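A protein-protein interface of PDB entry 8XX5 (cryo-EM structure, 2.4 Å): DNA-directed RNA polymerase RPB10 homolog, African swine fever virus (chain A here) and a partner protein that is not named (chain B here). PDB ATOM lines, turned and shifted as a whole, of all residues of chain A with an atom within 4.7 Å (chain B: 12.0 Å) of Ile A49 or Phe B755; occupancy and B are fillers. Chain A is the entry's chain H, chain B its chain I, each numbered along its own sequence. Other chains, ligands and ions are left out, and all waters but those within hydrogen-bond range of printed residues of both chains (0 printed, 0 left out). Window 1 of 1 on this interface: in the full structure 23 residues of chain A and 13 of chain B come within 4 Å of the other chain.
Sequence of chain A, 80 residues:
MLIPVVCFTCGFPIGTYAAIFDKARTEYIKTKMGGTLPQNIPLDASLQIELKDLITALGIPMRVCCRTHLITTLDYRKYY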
ATOM      1  N   TYR A  28      15.666 -15.172 -30.628  1.00  0.00           N
ATOM      2  CA  TYR A  28      15.022 -13.881 -30.840  1.00  0.00           C
ATOM      3  C   TYR A  28      16.047 -12.758 -30.918  1.00  0.00           C
ATOM      4  O   TYR A  28      15.914 -11.846 -31.740  1.00  0.00           O
ATOM      5  CB  TYR A  28      14.008 -13.624 -29.725  1.00  0.00           C
ATOM      6  CG  TYR A  28      13.506 -12.202 -29.632  1.00  0.00           C
ATOM      7  CD1 TYR A  28      12.431 -11.776 -30.398  1.00  0.00           C
ATOM      8  CD2 TYR A  28      14.092 -11.292 -28.763  1.00  0.00           C
ATOM      9  CE1 TYR A  28      11.964 -10.481 -30.311  1.00  0.00           C
ATOM     10  CE2 TYR A  28      13.632  -9.997 -28.672  1.00  0.00           C
ATOM     11  CZ  TYR A  28      12.567  -9.596 -29.447  1.00  0.00           C
ATOM     12  OH  TYR A  28      12.106  -8.304 -29.357  1.00  0.00           O
ATOM     13  N   ILE A  29      17.078 -12.809 -30.073  1.00  0.00           N
ATOM     14  CA  ILE A  29      18.114 -11.783 -30.084  1.00  0.00           C
ATOM     15  C   ILE A  29      18.874 -11.814 -31.402  1.00  0.00           C
ATOM     16  O   ILE A  29      19.224 -10.766 -31.956  1.00  0.00           O
ATOM     17  CB  ILE A  29      19.052 -11.962 -28.876  1.00  0.00           C
ATOM     18  CG1 ILE A  29      18.400 -11.403 -27.611  1.00  0.00           C
ATOM     19  CG2 ILE A  29      20.392 -11.291 -29.121  1.00  0.00           C
ATOM     20  CD1 ILE A  29      19.191 -11.666 -26.354  1.00  0.00           C
ATOM     21  N   LYS A  32      17.293  -9.580 -33.879  1.00  0.00           N
ATOM     22  CA  LYS A  32      17.259  -8.147 -33.620  1.00  0.00           C
ATOM     23  C   LYS A  32      18.617  -7.474 -33.725  1.00  0.00           C
ATOM     24  O   LYS A  32      18.676  -6.290 -34.054  1.00  0.00           O
ATOM     25  CB  LYS A  32      16.679  -7.863 -32.227  1.00  0.00           C
ATOM     26  CG  LYS A  32      15.522  -8.760 -31.834  1.00  0.00           C
ATOM     27  CD  LYS A  32      14.300  -8.507 -32.699  1.00  0.00           C
ATOM     28  CE  LYS A  32      13.757  -7.105 -32.488  1.00  0.00           C
ATOM     29  NZ  LYS A  32      12.386  -6.960 -33.044  1.00  0.00           N
ATOM     30  N   ILE A  41      26.331  -5.820 -27.847  1.00  0.00           N
ATOM     31  CA  ILE A  41      24.875  -5.704 -27.759  1.00  0.00           C
ATOM     32  C   ILE A  41      24.433  -4.819 -26.599  1.00  0.00           C
ATOM     33  O   ILE A  41      23.555  -3.965 -26.804  1.00  0.00           O
ATOM     34  CB  ILE A  41      24.238  -7.107 -27.717  1.00  0.00           C
ATOM     35  CG1 ILE A  41      24.169  -7.698 -29.126  1.00  0.00           C
ATOM     36  CG2 ILE A  41      22.858  -7.062 -27.083  1.00  0.00           C
ATOM     37  CD1 ILE A  41      23.580  -9.088 -29.173  1.00  0.00           C
ATOM     38  N   PRO A  42      24.979  -4.948 -25.383  1.00  0.00           N
ATOM     39  CA  PRO A  42      24.575  -4.030 -24.305  1.00  0.00           C
ATOM     40  C   PRO A  42      25.006  -2.588 -24.519  1.00  0.00           C
ATOM     41  O   PRO A  42      24.689  -1.738 -23.681  1.00  0.00           O
ATOM     42  CB  PRO A  42      25.259  -4.624 -23.063  1.00  0.00           C
ATOM     43  CG  PRO A  42      25.574  -6.024 -23.424  1.00  0.00           C
ATOM     44  CD  PRO A  42      25.888  -5.991 -24.874  1.00  0.00           C
ATOM     45  N   LEU A  43      25.715  -2.282 -25.603  1.00  0.00           N
ATOM     46  CA  LEU A  43      26.171  -0.929 -25.886  1.00  0.00           C
ATOM     47  C   LEU A  43      25.462  -0.297 -27.074  1.00  0.00           C
ATOM     48  O   LEU A  43      25.695   0.881 -27.360  1.00  0.00           O
ATOM     49  CB  LEU A  43      27.682  -0.927 -26.134  1.00  0.00           C
ATOM     50  CG  LEU A  43      28.570  -1.048 -24.898  1.00  0.00           C
ATOM     51  CD1 LEU A  43      29.845  -1.799 -25.239  1.00  0.00           C
ATOM     52  CD2 LEU A  43      28.885   0.327 -24.340  1.00  0.00           C
ATOM     53  N   ASP A  44      24.607  -1.041 -27.770  1.00  0.00           N
ATOM     54  CA  ASP A  44      23.960  -0.540 -28.975  1.00  0.00           C
ATOM     55  C   ASP A  44      22.792   0.359 -28.594  1.00  0.00           C
ATOM     56  O   ASP A  44      21.808  -0.105 -28.009  1.00  0.00           O
ATOM     57  CB  ASP A  44      23.490  -1.703 -29.846  1.00  0.00           C
ATOM     58  CG  ASP A  44      23.240  -1.290 -31.281  1.00  0.00           C
ATOM     59  OD1 ASP A  44      22.370  -0.426 -31.514  1.00  0.00           O
ATOM     60  OD2 ASP A  44      23.917  -1.831 -32.180  1.00  0.00           O
ATOM     61  N   LEU A  47      19.272  -0.668 -30.223  1.00  0.00           N
ATOM     62  CA  LEU A  47      18.631  -1.943 -29.941  1.00  0.00           C
ATOM     63  C   LEU A  47      17.406  -1.753 -29.058  1.00  0.00           C
ATOM     64  O   LEU A  47      17.422  -0.975 -28.099  1.00  0.00           O
ATOM     65  CB  LEU A  47      19.618  -2.893 -29.268  1.00  0.00           C
ATOM     66  CG  LEU A  47      20.452  -3.773 -30.198  1.00  0.00           C
ATOM     67  CD1 LEU A  47      21.109  -4.888 -29.414  1.00  0.00           C
ATOM     68  CD2 LEU A  47      19.595  -4.339 -31.319  1.00  0.00           C
ATOM     69  N   GLN A  48      16.331  -2.467 -29.393  1.00  0.00           N
ATOM     70  CA  GLN A  48      15.108  -2.488 -28.586  1.00  0.00           C
ATOM     71  C   GLN A  48      14.643  -3.941 -28.516  1.00  0.00           C
ATOM     72  O   GLN A  48      13.826  -4.381 -29.327  1.00  0.00           O
ATOM     73  CB  GLN A  48      14.038  -1.575 -29.167  1.00  0.00           C
ATOM     74  CG  GLN A  48      14.249  -0.108 -28.846  1.00  0.00           C
ATOM     75  CD  GLN A  48      12.961   0.684 -28.877  1.00  0.00           C
ATOM     76  OE1 GLN A  48      12.114   0.479 -29.744  1.00  0.00           O
ATOM     77  NE2 GLN A  48      12.805   1.596 -27.926  1.00  0.00           N
ATOM     78  N   ILE A  49      15.162  -4.673 -27.537  1.00  0.00           N
ATOM     79  CA  ILE A  49      14.869  -6.092 -27.376  1.00  0.00           C
ATOM     80  C   ILE A  49      13.878  -6.247 -26.233  1.00  0.00           C
ATOM     81  O   ILE A  49      14.189  -5.926 -25.080  1.00  0.00           O
ATOM     82  CB  ILE A  49      16.148  -6.903 -27.118  1.00  0.00           C
ATOM     83  CG1 ILE A  49      16.938  -7.073 -28.416  1.00  0.00           C
ATOM     84  CG2 ILE A  49      15.813  -8.259 -26.520  1.00  0.00           C
ATOM     85  CD1 ILE A  49      18.418  -7.273 -28.209  1.00  0.00           C
ATOM     86  N   GLU A  50      12.681  -6.730 -26.553  1.00  0.00           N
ATOM     87  CA  GLU A  50      11.626  -6.952 -25.576  1.00  0.00           C
ATOM     88  C   GLU A  50      11.326  -8.440 -25.503  1.00  0.00           C
ATOM     89  O   GLU A  50      11.099  -9.082 -26.533  1.00  0.00           O
ATOM     90  CB  GLU A  50      10.359  -6.177 -25.941  1.00  0.00           C
ATOM     91  CG  GLU A  50      10.479  -4.678 -25.769  1.00  0.00           C
ATOM     92  CD  GLU A  50       9.132  -4.008 -25.598  1.00  0.00           C
ATOM     93  OE1 GLU A  50       8.187  -4.683 -25.135  1.00  0.00           O
ATOM     94  OE2 GLU A  50       9.018  -2.808 -25.924  1.00  0.00           O
ATOM     95  N   LEU A  51      11.327  -8.984 -24.289  1.00  0.00           N
ATOM     96  CA  LEU A  51      11.060 -10.397 -24.066  1.00  0.00           C
ATOM     97  C   LEU A  51       9.687 -10.641 -23.459  1.00  0.00           C
ATOM     98  O   LEU A  51       9.387 -11.773 -23.068  1.00  0.00           O
ATOM     99  CB  LEU A  51      12.147 -11.000 -23.176  1.00  0.00           C
ATOM    100  CG  LEU A  51      13.560 -10.917 -23.753  1.00  0.00           C
ATOM    101  CD1 LEU A  51      14.597 -11.165 -22.672  1.00  0.00           C
ATOM    102  CD2 LEU A  51      13.723 -11.901 -24.900  1.00  0.00           C
ATOM    103  N   ALA B 748      29.755 -15.586 -26.593  1.00  0.00           N
ATOM    104  CA  ALA B 748      29.280 -14.289 -26.126  1.00  0.00           C
ATOM    105  C   ALA B 748      27.922 -13.952 -26.720  1.00  0.00           C
ATOM    106  O   ALA B 748      27.122 -13.261 -26.081  1.00  0.00           O
ATOM    107  CB  ALA B 748      30.296 -13.199 -26.465  1.00  0.00           C
ATOM    108  N   LEU B 749      27.648 -14.418 -27.940  1.00  0.00           N
ATOM    109  CA  LEU B 749      26.294 -14.304 -28.471  1.00  0.00           C
ATOM    110  C   LEU B 749      25.310 -15.094 -27.617  1.00  0.00           C
ATOM    111  O   LEU B 749      24.197 -14.629 -27.347  1.00  0.00           O
ATOM    112  CB  LEU B 749      26.250 -14.778 -29.923  1.00  0.00           C
ATOM    113  CG  LEU B 749      24.888 -14.763 -30.623  1.00  0.00           C
ATOM    114  CD1 LEU B 749      24.139 -13.467 -30.350  1.00  0.00           C
ATOM    115  CD2 LEU B 749      25.058 -14.977 -32.116  1.00  0.00           C
ATOM    116  N   LEU B 750      25.706 -16.291 -27.178  1.00  0.00           N
ATOM    117  CA  LEU B 750      24.830 -17.073 -26.310  1.00  0.00           C
ATOM    118  C   LEU B 750      24.620 -16.426 -24.945  1.00  0.00           C
ATOM    119  O   LEU B 750      23.625 -16.727 -24.280  1.00  0.00           O
ATOM    120  CB  LEU B 750      25.383 -18.485 -26.124  1.00  0.00           C
ATOM    121  CG  LEU B 750      25.583 -19.309 -27.393  1.00  0.00           C
ATOM    122  CD1 LEU B 750      26.109 -20.691 -27.051  1.00  0.00           C
ATOM    123  CD2 LEU B 750      24.283 -19.403 -28.171  1.00  0.00           C
ATOM    124  N   ALA B 751      25.518 -15.543 -24.517  1.00  0.00           N
ATOM    125  CA  ALA B 751      25.458 -14.956 -23.185  1.00  0.00           C
ATOM    126  C   ALA B 751      24.680 -13.648 -23.131  1.00  0.00           C
ATOM    127  O   ALA B 751      24.591 -13.043 -22.058  1.00  0.00           O
ATOM    128  CB  ALA B 751      26.873 -14.725 -22.647  1.00  0.00           C
ATOM    129  N   GLN B 752      24.119 -13.193 -24.247  1.00  0.00           N
ATOM    130  CA  GLN B 752      23.414 -11.919 -24.273  1.00  0.00           C
ATOM    131  C   GLN B 752      21.995 -12.073 -23.744  1.00  0.00           C
ATOM    132  O   GLN B 752      21.283 -13.018 -24.093  1.00  0.00           O
ATOM    133  CB  GLN B 752      23.390 -11.356 -25.692  1.00  0.00           C
ATOM    134  CG  GLN B 752      24.754 -10.931 -26.203  1.00  0.00           C
ATOM    135  CD  GLN B 752      25.567 -10.201 -25.153  1.00  0.00           C
ATOM    136  OE1 GLN B 752      25.167  -9.144 -24.668  1.00  0.00           O
ATOM    137  NE2 GLN B 752      26.715 -10.764 -24.798  1.00  0.00           N
ATOM    138  N   GLN B 753      21.585 -11.129 -22.896  1.00  0.00           N
ATOM    139  CA  GLN B 753      20.262 -11.144 -22.288  1.00  0.00           C
ATOM    140  C   GLN B 753      19.344 -10.058 -22.835  1.00  0.00           C
ATOM    141  O   GLN B 753      18.270  -9.828 -22.271  1.00  0.00           O
ATOM    142  CB  GLN B 753      20.377 -11.011 -20.768  1.00  0.00           C
ATOM    143  CG  GLN B 753      20.902 -12.257 -20.077  1.00  0.00           C
ATOM    144  CD  GLN B 753      21.388 -11.981 -18.671  1.00  0.00           C
ATOM    145  OE1 GLN B 753      21.995 -10.947 -18.405  1.00  0.00           O
ATOM    146  NE2 GLN B 753      21.122 -12.910 -17.763  1.00  0.00           N
ATOM    147  N   GLY B 754      19.737  -9.386 -23.915  1.00  0.00           N
ATOM    148  CA  GLY B 754      18.917  -8.335 -24.485  1.00  0.00           C
ATOM    149  C   GLY B 754      19.143  -7.003 -23.806  1.00  0.00           C
ATOM    150  O   GLY B 754      19.374  -6.956 -22.594  1.00  0.00           O
ATOM    151  N   PHE B 755      19.089  -5.909 -24.565  1.00  0.00           N
ATOM    152  CA  PHE B 755      19.412  -4.598 -24.021  1.00  0.00           C
ATOM    153  C   PHE B 755      18.223  -3.644 -24.008  1.00  0.00           C
ATOM    154  O   PHE B 755      17.814  -3.198 -22.936  1.00  0.00           O
ATOM    155  CB  PHE B 755      20.576  -3.997 -24.816  1.00  0.00           C
ATOM    156  CG  PHE B 755      20.970  -2.632 -24.361  1.00  0.00           C
ATOM    157  CD1 PHE B 755      21.001  -2.325 -23.015  1.00  0.00           C
ATOM    158  CD2 PHE B 755      21.306  -1.654 -25.276  1.00  0.00           C
ATOM    159  CE1 PHE B 755      21.356  -1.075 -22.594  1.00  0.00           C
ATOM    160  CE2 PHE B 755      21.668  -0.397 -24.856  1.00  0.00           C
ATOM    161  CZ  PHE B 755      21.692  -0.106 -23.515  1.00  0.00           C
ATOM    162  N   TYR B 756      17.645  -3.331 -25.169  1.00  0.00           N
ATOM    163  CA  TYR B 756      16.555  -2.363 -25.286  1.00  0.00           C
ATOM    164  C   TYR B 756      16.960  -0.947 -24.881  1.00  0.00           C
ATOM    165  O   TYR B 756      17.617  -0.738 -23.857  1.00  0.00           O
ATOM    166  CB  TYR B 756      15.337  -2.800 -24.467  1.00  0.00           C
ATOM    167  CG  TYR B 756      14.163  -1.853 -24.575  1.00  0.00           C
ATOM    168  CD1 TYR B 756      13.244  -1.972 -25.607  1.00  0.00           C
ATOM    169  CD2 TYR B 756      13.972  -0.840 -23.643  1.00  0.00           C
ATOM    170  CE1 TYR B 756      12.174  -1.111 -25.712  1.00  0.00           C
ATOM    171  CE2 TYR B 756      12.904   0.025 -23.741  1.00  0.00           C
ATOM    172  CZ  TYR B 756      12.008  -0.116 -24.778  1.00  0.00           C
ATOM    173  OH  TYR B 756      10.939   0.742 -24.881  1.00  0.00           O
ATOM    174  N   ASN B 757      16.554   0.036 -25.680  1.00  0.00           N
ATOM    175  CA  ASN B 757      16.761   1.446 -25.382  1.00  0.00           C
ATOM    176  C   ASN B 757      15.420   2.163 -25.385  1.00  0.00           C
ATOM    177  O   ASN B 757      14.580   1.922 -26.256  1.00  0.00           O
ATOM    178  CB  ASN B 757      17.696   2.102 -26.401  1.00  0.00           C
ATOM    179  CG  ASN B 757      19.109   1.574 -26.321  1.00  0.00           C
ATOM    180  OD1 ASN B 757      19.983   2.196 -25.721  1.00  0.00           O
ATOM    181  ND2 ASN B 757      19.342   0.418 -26.930  1.00  0.00           N
ATOM    182  N   ILE B 758      15.220   3.045 -24.409  1.00  0.00           N
ATOM    183  CA  ILE B 758      14.002   3.846 -24.370  1.00  0.00           C
ATOM    184  C   ILE B 758      14.097   4.918 -25.447  1.00  0.00           C
ATOM    185  O   ILE B 758      15.036   5.721 -25.463  1.00  0.00           O
ATOM    186  CB  ILE B 758      13.790   4.463 -22.983  1.00  0.00           C
ATOM    187  CG1 ILE B 758      13.379   3.388 -21.976  1.00  0.00           C
ATOM    188  CG2 ILE B 758      12.740   5.559 -23.042  1.00  0.00           C
ATOM    189  CD1 ILE B 758      13.987   3.567 -20.607  1.00  0.00           C
ATOM    190  N   PHE B 759      13.125   4.934 -26.352  1.00  0.00           N
ATOM    191  CA  PHE B 759      13.150   5.819 -27.506  1.00  0.00           C
ATOM    192  C   PHE B 759      12.245   7.021 -27.288  1.00  0.00           C
ATOM    193  O   PHE B 759      11.169   6.907 -26.694  1.00  0.00           O
ATOM    194  CB  PHE B 759      12.717   5.079 -28.774  1.00  0.00           C
ATOM    195  CG  PHE B 759      13.827   4.331 -29.450  1.00  0.00           C
ATOM    196  CD1 PHE B 759      15.065   4.206 -28.847  1.00  0.00           C
ATOM    197  CD2 PHE B 759      13.630   3.752 -30.690  1.00  0.00           C
ATOM    198  CE1 PHE B 759      16.085   3.517 -29.466  1.00  0.00           C
ATOM    199  CE2 PHE B 759      14.648   3.062 -31.315  1.00  0.00           C
ATOM    200  CZ  PHE B 759      15.876   2.944 -30.703  1.00  0.00           C
ATOM    201  N   ARG B 765      15.192   7.604 -31.717  1.00  0.00           N
ATOM    202  CA  ARG B 765      16.534   7.307 -31.243  1.00  0.00           C
ATOM    203  C   ARG B 765      16.492   7.254 -29.724  1.00  0.00           C
ATOM    204  O   ARG B 765      15.430   7.385 -29.110  1.00  0.00           O
ATOM    205  CB  ARG B 765      17.541   8.349 -31.740  1.00  0.00           C
ATOM    206  CG  ARG B 765      18.027   8.112 -33.157  1.00  0.00           C
ATOM    207  CD  ARG B 765      18.841   9.289 -33.666  1.00  0.00           C
ATOM    208  NE  ARG B 765      18.001  10.289 -34.313  1.00  0.00           N
ATOM    209  CZ  ARG B 765      17.637  11.435 -33.755  1.00  0.00           C
ATOM    210  NH1 ARG B 765      18.028  11.766 -32.536  1.00  0.00           N
ATOM    211  NH2 ARG B 765      16.861  12.271 -34.439  1.00  0.00           N
ATOM    212  N   ALA B 766      17.659   7.063 -29.113  1.00  0.00           N
ATOM    213  CA  ALA B 766      17.743   7.033 -27.661  1.00  0.00           C
ATOM    214  C   ALA B 766      17.193   8.327 -27.077  1.00  0.00           C
ATOM    215  O   ALA B 766      17.508   9.421 -27.554  1.00  0.00           O
ATOM    216  CB  ALA B 766      19.190   6.821 -27.217  1.00  0.00           C
ATOM    217  N   ASP B 767      16.355   8.196 -26.052  1.00  0.00           N
ATOM    218  CA  ASP B 767      15.690   9.354 -25.469  1.00  0.00           C
ATOM    219  C   ASP B 767      16.710  10.311 -24.873  1.00  0.00           C
ATOM    220  O   ASP B 767      17.506   9.930 -24.010  1.00  0.00           O
ATOM    221  CB  ASP B 767      14.694   8.901 -24.404  1.00  0.00           C
ATOM    222  CG  ASP B 767      13.605   9.925 -24.148  1.00  0.00           C
ATOM    223  OD1 ASP B 767      13.792  11.102 -24.516  1.00  0.00           O
ATOM    224  OD2 ASP B 767      12.559   9.549 -23.581  1.00  0.00           O
ATOM    225  N   GLN B 768      16.686  11.558 -25.339  1.00  0.00           N
ATOM    226  CA  GLN B 768      17.581  12.594 -24.850  1.00  0.00           C
ATOM    227  C   GLN B 768      16.854  13.682 -24.078  1.00  0.00           C
ATOM    228  O   GLN B 768      17.498  14.633 -23.624  1.00  0.00           O
ATOM    229  CB  GLN B 768      18.354  13.220 -26.017  1.00  0.00           C
ATOM    230  CG  GLN B 768      19.183  12.233 -26.817  1.00  0.00           C
ATOM    231  CD  GLN B 768      20.377  11.716 -26.043  1.00  0.00           C
ATOM    232  OE1 GLN B 768      20.491  10.519 -25.783  1.00  0.00           O
ATOM    233  NE2 GLN B 768      21.274  12.618 -25.669  1.00  0.00           N
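Hydrophobic or aromatic side chains of chain B within 4 Å of the printed part of chain A: Phe B755, Tyr B756 and Phe B759.
Along chain B the printed residues that touch a printed residue of chain A span positions 752 to 759.
Printed residues of chain A that touch a printed residue of chain B: Ile A29, Ile A41, Pro A42, Asp A44, Leu A47, Gln A48, Ile A49, Glu A50 and Leu A51.
Among the printed residues, pairs that only touch across the chains: Ile A29 with Gln B752 (3.4 Å), Ile A29 with Gln B753 (3.9 Å), Ile A29 with Gly B754 (3.4 Å), Ile A41 with Gln B752 (3.7 Å), Ile A41 with Phe B755 (3.6 Å), Pro A42 with Gln B752 (3.2 Å), Pro A42 with Phe B755 (3.4 Å), Asp A44 with Phe B755 (3.2 Å), Leu A47 with Tyr B756 (3.3 Å), Gln A48 with Tyr B756 (3.6 Å), Gln A48 with Phe B759 (3.3 Å), Ile A49 with Gly B754 (3.7 Å), Ile A49 with Phe B755 (3.9 Å), Ile A49 with Tyr B756 (3.4 Å), Glu A50 with Tyr B756 (3.6 Å) and Leu A51 with Gln B753 (3.9 Å).
Of chain B, only Gln B752 (3.4 Å), Gln B753 (3.9 Å) and Gly B754 (3.4 Å) come within 4 Å of Ile A29.
Lys A32 touches none of the printed residues of chain B.
Printed residues of chain B within 4 Å of Ile A41: Gln B752 and Phe B755.
Printed residues of chain B within 4 Å of Asp A44: Phe B755 and Asn B757.
Of chain B, only Tyr B756 (3.3 Å) and Asn B757 (2.6 Å) come within 4 Å of Leu A47.
Of chain B, only Tyr B756, Asn B757 and Phe B759 come within 4 Å of Gln A48.
Ile A49 touches just these residues of chain B: Gly B754 (3.7 Å), Phe B755 (3.9 Å) and Tyr B756 (3.4 Å).
Of chain B, only Gln B753 comes within 4 Å of Leu A51.
Of the printed residues of chain A, Gln B753 touches Ile A29 (3.9 Å) and Leu A51 (3.9 Å).
Phe B755 touches just these residues of chain A: Ile A41, Pro A42, Asp A44 and Ile A49.
Of the printed residues of chain A, Tyr B756 touches Leu A47, Gln A48, Ile A49 and Glu A50.
The nearest residue of chain B that does not touch Ile A49 is Gln B753 (5.2 Å).
The backbone NH (N) of Leu A47 sits at hydrogen-bond distance from the side-chain carboxylate (OD1) of Asp A44, at 3.4 Å.
The side-chain hydroxyl of Tyr A28 is in hydrogen-bond range of the backbone carbonyl oxygen of Glu A50 (3.1 Å).
NE2 of Gln B752 lies within hydrogen-bond range of O of Ala B748, at 2.8 Å.
The backbone carbonyl oxygen of Asp A44 sits at hydrogen-bond distance from the side-chain amide nitrogen of Asn B757, 2.7 Å away.
NE2 of Gln A48 is in hydrogen-bond range of O of Asn B757.
The backbone carbonyl oxygen (O) of Leu A47 is in hydrogen-bond range of the side-chain amide nitrogen (ND2) of Asn B757 (2.6 Å).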
